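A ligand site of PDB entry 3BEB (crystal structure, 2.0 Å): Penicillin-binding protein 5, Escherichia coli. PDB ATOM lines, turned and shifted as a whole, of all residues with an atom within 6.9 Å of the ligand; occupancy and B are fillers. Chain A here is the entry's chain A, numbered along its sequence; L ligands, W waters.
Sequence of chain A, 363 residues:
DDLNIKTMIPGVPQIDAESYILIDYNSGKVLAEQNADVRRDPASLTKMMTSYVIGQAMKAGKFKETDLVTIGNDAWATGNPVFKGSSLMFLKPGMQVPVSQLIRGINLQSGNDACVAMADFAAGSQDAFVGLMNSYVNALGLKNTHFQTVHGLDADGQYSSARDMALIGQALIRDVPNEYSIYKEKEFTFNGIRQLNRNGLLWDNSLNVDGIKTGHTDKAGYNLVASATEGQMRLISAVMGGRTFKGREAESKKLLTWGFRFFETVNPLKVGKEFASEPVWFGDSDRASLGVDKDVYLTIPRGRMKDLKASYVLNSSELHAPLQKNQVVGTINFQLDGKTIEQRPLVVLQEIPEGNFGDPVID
O of His 216 lies within hydrogen-bond range of N1 of the ligand (3.0 Å).
The backbone NH (N) of His 216 is in hydrogen-bond range of an oxygen (O2) of the ligand, at 2.9 Å.
The side-chain hydroxyl (OG) of Ser 44 is bonded to a carbon (C5) of the ligand (1.4 Å).
An oxygen (O2) of the ligand sits close to the backbone NH (N) of Ser 44, 2.9 Å away.
ND2 of Asn 112 sits at hydrogen-bond distance from OG of Ser 86, 3.2 Å away.
O of Gln 109 is in hydrogen-bond range of NE of Arg 198.
The guanidinium group (NH2) of Arg 198 sits at hydrogen-bond distance from the side-chain hydroxyl (OG) of Ser 87, at 3.0 Å.
The backbone carbonyl oxygen (O) of Gly 215 sits at hydrogen-bond distance from the backbone NH (N) of Asn 223, 2.6 Å away.
Merely in contact with the ligand: Ala 43 (3.4 Å), Ser 86 (3.6 Å), Arg 198 (3.1 Å), Thr 214 (2.9 Å), Gly 215 (3.3 Å) and Thr 217 (3.97 Å).
Within 4 Å of the ligand: Ala 43, Ser 44, Ser 86, Arg 198, Thr 214, Gly 215, His 216 and Thr 217.
Water W1 lies within hydrogen-bond range of the side-chain amide nitrogen of Asn 112 (2.8 Å), the backbone carbonyl oxygen of Ser 110 (3.0 Å), the backbone NH of Ser 87 (3.0 Å) and an oxygen (O1) of the ligand (3.5 Å).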
ATOM      1  N   PRO A  42      17.512 -17.845 -26.650  1.00  0.00           N
ATOM      2  CA  PRO A  42      18.121 -18.548 -27.786  1.00  0.00           C
ATOM      3  C   PRO A  42      17.787 -20.051 -27.885  1.00  0.00           C
ATOM      4  O   PRO A  42      18.235 -20.703 -28.822  1.00  0.00           O
ATOM      5  CB  PRO A  42      19.638 -18.334 -27.584  1.00  0.00           C
ATOM      6  CG  PRO A  42      19.793 -18.130 -26.079  1.00  0.00           C
ATOM      7  CD  PRO A  42      18.455 -17.663 -25.526  1.00  0.00           C
ATOM      8  N   ALA A  43      17.017 -20.601 -26.936  1.00  0.00           N
ATOM      9  CA  ALA A  43      16.711 -22.041 -26.990  1.00  0.00           C
ATOM     10  C   ALA A  43      17.998 -22.839 -27.263  1.00  0.00           C
ATOM     11  O   ALA A  43      19.029 -22.577 -26.634  1.00  0.00           O
ATOM     12  CB  ALA A  43      15.663 -22.317 -28.042  1.00  0.00           C
ATOM     13  N   SER A  44      17.934 -23.774 -28.215  1.00  0.00           N
ATOM     14  CA  SER A  44      19.059 -24.652 -28.580  1.00  0.00           C
ATOM     15  C   SER A  44      20.193 -23.945 -29.292  1.00  0.00           C
ATOM     16  O   SER A  44      21.255 -24.533 -29.470  1.00  0.00           O
ATOM     17  CB  SER A  44      18.582 -25.800 -29.451  1.00  0.00           C
ATOM     18  OG  SER A  44      17.842 -26.741 -28.701  1.00  0.00           O
ATOM     19  N   LEU A  45      19.971 -22.734 -29.755  1.00  0.00           N
ATOM     20  CA  LEU A  45      21.078 -21.975 -30.357  1.00  0.00           C
ATOM     21  C   LEU A  45      22.215 -21.785 -29.343  1.00  0.00           C
ATOM     22  O   LEU A  45      23.344 -21.490 -29.717  1.00  0.00           O
ATOM     23  CB  LEU A  45      20.598 -20.627 -30.915  1.00  0.00           C
ATOM     24  CG  LEU A  45      19.493 -20.523 -31.989  1.00  0.00           C
ATOM     25  CD1 LEU A  45      19.471 -19.147 -32.706  1.00  0.00           C
ATOM     26  CD2 LEU A  45      19.561 -21.625 -33.010  1.00  0.00           C
ATOM     27  N   LYS A  47      23.758 -24.095 -27.733  1.00  0.00           N
ATOM     28  CA  LYS A  47      24.768 -25.133 -28.095  1.00  0.00           C
ATOM     29  C   LYS A  47      25.737 -24.801 -29.244  1.00  0.00           C
ATOM     30  O   LYS A  47      26.656 -25.583 -29.524  1.00  0.00           O
ATOM     31  CB  LYS A  47      24.136 -26.499 -28.342  1.00  0.00           C
ATOM     32  CG  LYS A  47      23.160 -26.902 -27.255  1.00  0.00           C
ATOM     33  CD  LYS A  47      22.418 -28.158 -27.607  1.00  0.00           C
ATOM     34  CE  LYS A  47      21.433 -28.516 -26.515  1.00  0.00           C
ATOM     35  NZ  LYS A  47      20.725 -27.311 -25.952  1.00  0.00           N
ATOM     36  N   LYS A  84      13.841 -33.516 -19.006  1.00  0.00           N
ATOM     37  CA  LYS A  84      12.487 -33.950 -19.453  1.00  0.00           C
ATOM     38  C   LYS A  84      11.950 -33.202 -20.689  1.00  0.00           C
ATOM     39  O   LYS A  84      11.839 -31.985 -20.697  1.00  0.00           O
ATOM     40  CB  LYS A  84      11.473 -33.841 -18.300  1.00  0.00           C
ATOM     41  CG  LYS A  84      10.060 -34.332 -18.655  1.00  0.00           C
ATOM     42  CD  LYS A  84       9.077 -34.228 -17.483  1.00  0.00           C
ATOM     43  CE  LYS A  84       8.855 -32.790 -17.072  1.00  0.00           C
ATOM     44  NZ  LYS A  84       8.069 -32.652 -15.802  1.00  0.00           N
ATOM     45  N   GLY A  85      11.636 -33.948 -21.737  1.00  0.00           N
ATOM     46  CA  GLY A  85      11.095 -33.409 -22.984  1.00  0.00           C
ATOM     47  C   GLY A  85      12.139 -32.955 -23.993  1.00  0.00           C
ATOM     48  O   GLY A  85      11.801 -32.647 -25.141  1.00  0.00           O
ATOM     49  N   SER A  86      13.408 -32.922 -23.567  1.00  0.00           N
ATOM     50  CA  SER A  86      14.488 -32.351 -24.376  1.00  0.00           C
ATOM     51  C   SER A  86      15.229 -33.396 -25.216  1.00  0.00           C
ATOM     52  O   SER A  86      15.117 -34.598 -24.965  1.00  0.00           O
ATOM     53  CB  SER A  86      15.470 -31.561 -23.498  1.00  0.00           C
ATOM     54  OG  SER A  86      16.268 -32.413 -22.680  1.00  0.00           O
ATOM     55  N   SER A  87      15.965 -32.922 -26.214  1.00  0.00           N
ATOM     56  CA  SER A  87      16.739 -33.790 -27.077  1.00  0.00           C
ATOM     57  C   SER A  87      17.823 -34.396 -26.209  1.00  0.00           C
ATOM     58  O   SER A  87      18.422 -33.702 -25.381  1.00  0.00           O
ATOM     59  CB  SER A  87      17.321 -32.988 -28.237  1.00  0.00           C
ATOM     60  OG  SER A  87      18.107 -33.807 -29.092  1.00  0.00           O
ATOM     61  N   GLN A 109      22.334 -33.300 -33.121  1.00  0.00           N
ATOM     62  CA  GLN A 109      21.146 -33.687 -32.364  1.00  0.00           C
ATOM     63  C   GLN A 109      20.776 -32.724 -31.233  1.00  0.00           C
ATOM     64  O   GLN A 109      19.686 -32.806 -30.683  1.00  0.00           O
ATOM     65  CB  GLN A 109      21.387 -35.094 -31.817  1.00  0.00           C
ATOM     66  CG  GLN A 109      20.186 -35.763 -31.147  1.00  0.00           C
ATOM     67  CD  GLN A 109      20.553 -37.116 -30.592  1.00  0.00           C
ATOM     68  OE1 GLN A 109      21.685 -37.582 -30.754  1.00  0.00           O
ATOM     69  NE2 GLN A 109      19.588 -37.770 -29.922  1.00  0.00           N
ATOM     70  N   SER A 110      21.682 -31.818 -30.876  1.00  0.00           N
ATOM     71  CA  SER A 110      21.475 -30.932 -29.716  1.00  0.00           C
ATOM     72  C   SER A 110      21.181 -31.717 -28.417  1.00  0.00           C
ATOM     73  O   SER A 110      20.435 -31.244 -27.575  1.00  0.00           O
ATOM     74  CB  SER A 110      20.388 -29.881 -30.010  1.00  0.00           C
ATOM     75  OG  SER A 110      20.784 -28.933 -31.006  1.00  0.00           O
ATOM     76  N   ASN A 112      21.318 -32.680 -24.908  1.00  0.00           N
ATOM     77  CA  ASN A 112      21.697 -31.881 -23.752  1.00  0.00           C
ATOM     78  C   ASN A 112      22.508 -32.659 -22.770  1.00  0.00           C
ATOM     79  O   ASN A 112      23.331 -32.088 -22.052  1.00  0.00           O
ATOM     80  CB  ASN A 112      20.469 -31.364 -23.016  1.00  0.00           C
ATOM     81  CG  ASN A 112      19.633 -30.482 -23.872  1.00  0.00           C
ATOM     82  OD1 ASN A 112      19.915 -29.286 -24.032  1.00  0.00           O
ATOM     83  ND2 ASN A 112      18.598 -31.056 -24.456  1.00  0.00           N
ATOM     84  N   HIS A 151      23.785 -26.104 -21.866  1.00  0.00           N
ATOM     85  CA  HIS A 151      22.808 -26.629 -22.828  1.00  0.00           C
ATOM     86  C   HIS A 151      21.755 -25.595 -23.191  1.00  0.00           C
ATOM     87  O   HIS A 151      21.159 -25.652 -24.266  1.00  0.00           O
ATOM     88  CB  HIS A 151      22.097 -27.899 -22.294  1.00  0.00           C
ATOM     89  CG  HIS A 151      21.965 -27.959 -20.797  1.00  0.00           C
ATOM     90  ND1 HIS A 151      21.432 -26.920 -20.042  1.00  0.00           N
ATOM     91  CD2 HIS A 151      22.247 -28.947 -19.921  1.00  0.00           C
ATOM     92  CE1 HIS A 151      21.445 -27.262 -18.763  1.00  0.00           C
ATOM     93  NE2 HIS A 151      21.924 -28.491 -18.666  1.00  0.00           N
ATOM     94  N   LEU A 153      19.178 -25.141 -21.126  1.00  0.00           N
ATOM     95  CA  LEU A 153      18.050 -25.459 -20.249  1.00  0.00           C
ATOM     96  C   LEU A 153      18.342 -24.840 -18.912  1.00  0.00           C
ATOM     97  O   LEU A 153      19.494 -24.522 -18.593  1.00  0.00           O
ATOM     98  CB  LEU A 153      17.882 -26.966 -20.035  1.00  0.00           C
ATOM     99  CG  LEU A 153      17.683 -27.905 -21.208  1.00  0.00           C
ATOM    100  CD1 LEU A 153      18.011 -29.328 -20.746  1.00  0.00           C
ATOM    101  CD2 LEU A 153      16.284 -27.801 -21.802  1.00  0.00           C
ATOM    102  N   ARG A 198      18.719 -32.133 -37.463  1.00  0.00           N
ATOM    103  CA  ARG A 198      17.431 -31.404 -37.461  1.00  0.00           C
ATOM    104  C   ARG A 198      17.401 -30.179 -38.375  1.00  0.00           C
ATOM    105  O   ARG A 198      16.350 -29.593 -38.591  1.00  0.00           O
ATOM    106  CB  ARG A 198      17.002 -31.027 -36.033  1.00  0.00           C
ATOM    107  CG  ARG A 198      16.923 -32.181 -35.016  1.00  0.00           C
ATOM    108  CD  ARG A 198      16.868 -31.637 -33.570  1.00  0.00           C
ATOM    109  NE  ARG A 198      16.934 -32.675 -32.533  1.00  0.00           N
ATOM    110  CZ  ARG A 198      15.921 -33.475 -32.188  1.00  0.00           C
ATOM    111  NH1 ARG A 198      14.741 -33.384 -32.802  1.00  0.00           N
ATOM    112  NH2 ARG A 198      16.076 -34.398 -31.241  1.00  0.00           N
ATOM    113  N   ASN A 199      18.552 -29.777 -38.921  1.00  0.00           N
ATOM    114  CA  ASN A 199      18.576 -28.718 -39.934  1.00  0.00           C
ATOM    115  C   ASN A 199      18.169 -29.267 -41.307  1.00  0.00           C
ATOM    116  O   ASN A 199      18.985 -29.814 -42.038  1.00  0.00           O
ATOM    117  CB  ASN A 199      19.957 -28.034 -39.979  1.00  0.00           C
ATOM    118  CG  ASN A 199      20.008 -26.804 -40.886  1.00  0.00           C
ATOM    119  OD1 ASN A 199      18.998 -26.389 -41.480  1.00  0.00           O
ATOM    120  ND2 ASN A 199      21.194 -26.229 -40.995  1.00  0.00           N
ATOM    121  N   THR A 214      19.460 -25.204 -35.379  1.00  0.00           N
ATOM    122  CA  THR A 214      18.013 -25.115 -35.272  1.00  0.00           C
ATOM    123  C   THR A 214      17.637 -25.055 -33.771  1.00  0.00           C
ATOM    124  O   THR A 214      18.397 -25.498 -32.905  1.00  0.00           O
ATOM    125  CB  THR A 214      17.437 -26.378 -35.970  1.00  0.00           C
ATOM    126  OG1 THR A 214      16.132 -26.121 -36.495  1.00  0.00           O
ATOM    127  CG2 THR A 214      17.407 -27.557 -35.021  1.00  0.00           C
ATOM    128  N   GLY A 215      16.478 -24.490 -33.460  1.00  0.00           N
ATOM    129  CA  GLY A 215      16.078 -24.345 -32.051  1.00  0.00           C
ATOM    130  C   GLY A 215      14.619 -23.944 -31.890  1.00  0.00           C
ATOM    131  O   GLY A 215      14.100 -23.207 -32.704  1.00  0.00           O
ATOM    132  N   HIS A 216      13.963 -24.467 -30.864  1.00  0.00           N
ATOM    133  CA  HIS A 216      12.562 -24.165 -30.598  1.00  0.00           C
ATOM    134  C   HIS A 216      12.198 -24.442 -29.152  1.00  0.00           C
ATOM    135  O   HIS A 216      12.570 -25.483 -28.604  1.00  0.00           O
ATOM    136  CB  HIS A 216      11.601 -24.949 -31.510  1.00  0.00           C
ATOM    137  CG  HIS A 216      10.153 -24.702 -31.185  1.00  0.00           C
ATOM    138  ND1 HIS A 216       9.428 -25.532 -30.355  1.00  0.00           N
ATOM    139  CD2 HIS A 216       9.315 -23.696 -31.533  1.00  0.00           C
ATOM    140  CE1 HIS A 216       8.199 -25.050 -30.218  1.00  0.00           C
ATOM    141  NE2 HIS A 216       8.113 -23.937 -30.930  1.00  0.00           N
ATOM    142  N   THR A 217      11.522 -23.480 -28.539  1.00  0.00           N
ATOM    143  CA  THR A 217      10.794 -23.630 -27.286  1.00  0.00           C
ATOM    144  C   THR A 217       9.518 -22.792 -27.448  1.00  0.00           C
ATOM    145  O   THR A 217       9.437 -21.979 -28.371  1.00  0.00           O
ATOM    146  CB  THR A 217      11.583 -23.110 -26.075  1.00  0.00           C
ATOM    147  OG1 THR A 217      11.863 -21.730 -26.245  1.00  0.00           O
ATOM    148  CG2 THR A 217      12.906 -23.846 -25.896  1.00  0.00           C
ATOM    149  N   ASP A 218       8.528 -22.993 -26.573  1.00  0.00           N
ATOM    150  CA  ASP A 218       7.295 -22.215 -26.653  1.00  0.00           C
ATOM    151  C   ASP A 218       7.556 -20.741 -26.385  1.00  0.00           C
ATOM    152  O   ASP A 218       6.988 -19.892 -27.057  1.00  0.00           O
ATOM    153  CB  ASP A 218       6.206 -22.753 -25.704  1.00  0.00           C
ATOM    154  CG  ASP A 218       5.436 -23.933 -26.293  1.00  0.00           C
ATOM    155  OD1 ASP A 218       5.162 -23.935 -27.512  1.00  0.00           O
ATOM    156  OD2 ASP A 218       5.077 -24.842 -25.529  1.00  0.00           O
ATOM    157  N   GLY A 221       9.908 -19.613 -29.616  1.00  0.00           N
ATOM    158  CA  GLY A 221       9.455 -19.798 -31.001  1.00  0.00           C
ATOM    159  C   GLY A 221      10.494 -20.602 -31.763  1.00  0.00           C
ATOM    160  O   GLY A 221      11.268 -21.299 -31.152  1.00  0.00           O
ATOM    161  N   TYR A 222      10.492 -20.498 -33.093  1.00  0.00           N
ATOM    162  CA  TYR A 222      11.433 -21.247 -33.934  1.00  0.00           C
ATOM    163  C   TYR A 222      12.671 -20.429 -34.271  1.00  0.00           C
ATOM    164  O   TYR A 222      12.588 -19.312 -34.777  1.00  0.00           O
ATOM    165  CB  TYR A 222      10.741 -21.725 -35.216  1.00  0.00           C
ATOM    166  CG  TYR A 222       9.653 -22.715 -34.935  1.00  0.00           C
ATOM    167  CD1 TYR A 222       8.343 -22.295 -34.708  1.00  0.00           C
ATOM    168  CD2 TYR A 222       9.932 -24.075 -34.873  1.00  0.00           C
ATOM    169  CE1 TYR A 222       7.322 -23.207 -34.421  1.00  0.00           C
ATOM    170  CE2 TYR A 222       8.920 -25.007 -34.590  1.00  0.00           C
ATOM    171  CZ  TYR A 222       7.619 -24.558 -34.365  1.00  0.00           C
ATOM    172  OH  TYR A 222       6.630 -25.469 -34.083  1.00  0.00           O
ATOM    173  N   ASN A 223      13.844 -20.989 -33.956  1.00  0.00           N
ATOM    174  CA  ASN A 223      15.121 -20.358 -34.280  1.00  0.00           C
ATOM    175  C   ASN A 223      15.880 -21.182 -35.315  1.00  0.00           C
ATOM    176  O   ASN A 223      15.836 -22.409 -35.299  1.00  0.00           O
ATOM    177  CB  ASN A 223      16.007 -20.171 -33.030  1.00  0.00           C
ATOM    178  CG  ASN A 223      15.335 -19.374 -31.907  1.00  0.00           C
ATOM    179  OD1 ASN A 223      14.492 -18.523 -32.147  1.00  0.00           O
ATOM    180  ND2 ASN A 223      15.761 -19.632 -30.691  1.00  0.00           N
ATOM    181  N   ARG A 248       9.930 -22.177 -40.456  1.00  0.00           N
ATOM    182  CA  ARG A 248      11.257 -22.232 -39.869  1.00  0.00           C
ATOM    183  C   ARG A 248      12.377 -22.143 -40.922  1.00  0.00           C
ATOM    184  O   ARG A 248      13.235 -21.244 -40.888  1.00  0.00           O
ATOM    185  CB  ARG A 248      11.395 -23.529 -39.059  1.00  0.00           C
ATOM    186  CG  ARG A 248      10.959 -24.834 -39.785  1.00  0.00           C
ATOM    187  CD  ARG A 248      10.367 -25.833 -38.793  1.00  0.00           C
ATOM    188  NE  ARG A 248      10.796 -27.224 -39.016  1.00  0.00           N
ATOM    189  CZ  ARG A 248      10.174 -28.104 -39.806  1.00  0.00           C
ATOM    190  NH1 ARG A 248       9.110 -27.734 -40.497  1.00  0.00           N
ATOM    191  NH2 ARG A 248      10.630 -29.335 -39.942  1.00  0.00           N
HETATM  192  O1  LIG L   1      14.849 -28.795 -25.749  1.00  0.00           O
HETATM  193  C1  LIG L   1      14.089 -28.140 -26.455  1.00  0.00           C
HETATM  194  C2  LIG L   1      12.695 -27.815 -25.937  1.00  0.00           C
HETATM  195  C3  LIG L   1      11.622 -28.209 -26.924  1.00  0.00           C
HETATM  196  N1  LIG L   1      14.423 -27.685 -27.668  1.00  0.00           N
HETATM  197  C4  LIG L   1      15.763 -27.947 -28.223  1.00  0.00           C
HETATM  198  C5  LIG L   1      16.451 -26.678 -28.642  1.00  0.00           C
HETATM  199  O2  LIG L   1      15.824 -25.648 -28.906  1.00  0.00           O
HETATM  200  C6  LIG L   1      15.760 -28.937 -29.409  1.00  0.00           C
HETATM  201  S1  LIG L   1      14.384 -30.050 -29.364  1.00  0.00           S
HETATM  202  N2  LIG L   1      15.699 -28.271 -30.698  1.00  0.00           N
HETATM  203  C7  LIG L   1      14.377 -28.207 -31.294  1.00  0.00           C
HETATM  204  C8  LIG L   1      14.359 -27.835 -32.773  1.00  0.00           C
HETATM  205  O3  LIG L   1      13.657 -26.868 -33.119  1.00  0.00           O
HETATM  206  O4  LIG L   1      15.069 -28.440 -33.604  1.00  0.00           O
HETATM  207  C9  LIG L   1      13.626 -29.486 -30.870  1.00  0.00           C
HETATM  208  C10 LIG L   1      12.160 -29.119 -30.595  1.00  0.00           C
HETATM  209  C11 LIG L   1      13.654 -30.612 -31.907  1.00  0.00           C
HETATM  210  O   HOH W   1      17.625 -30.482 -26.964  1.00  0.00           O
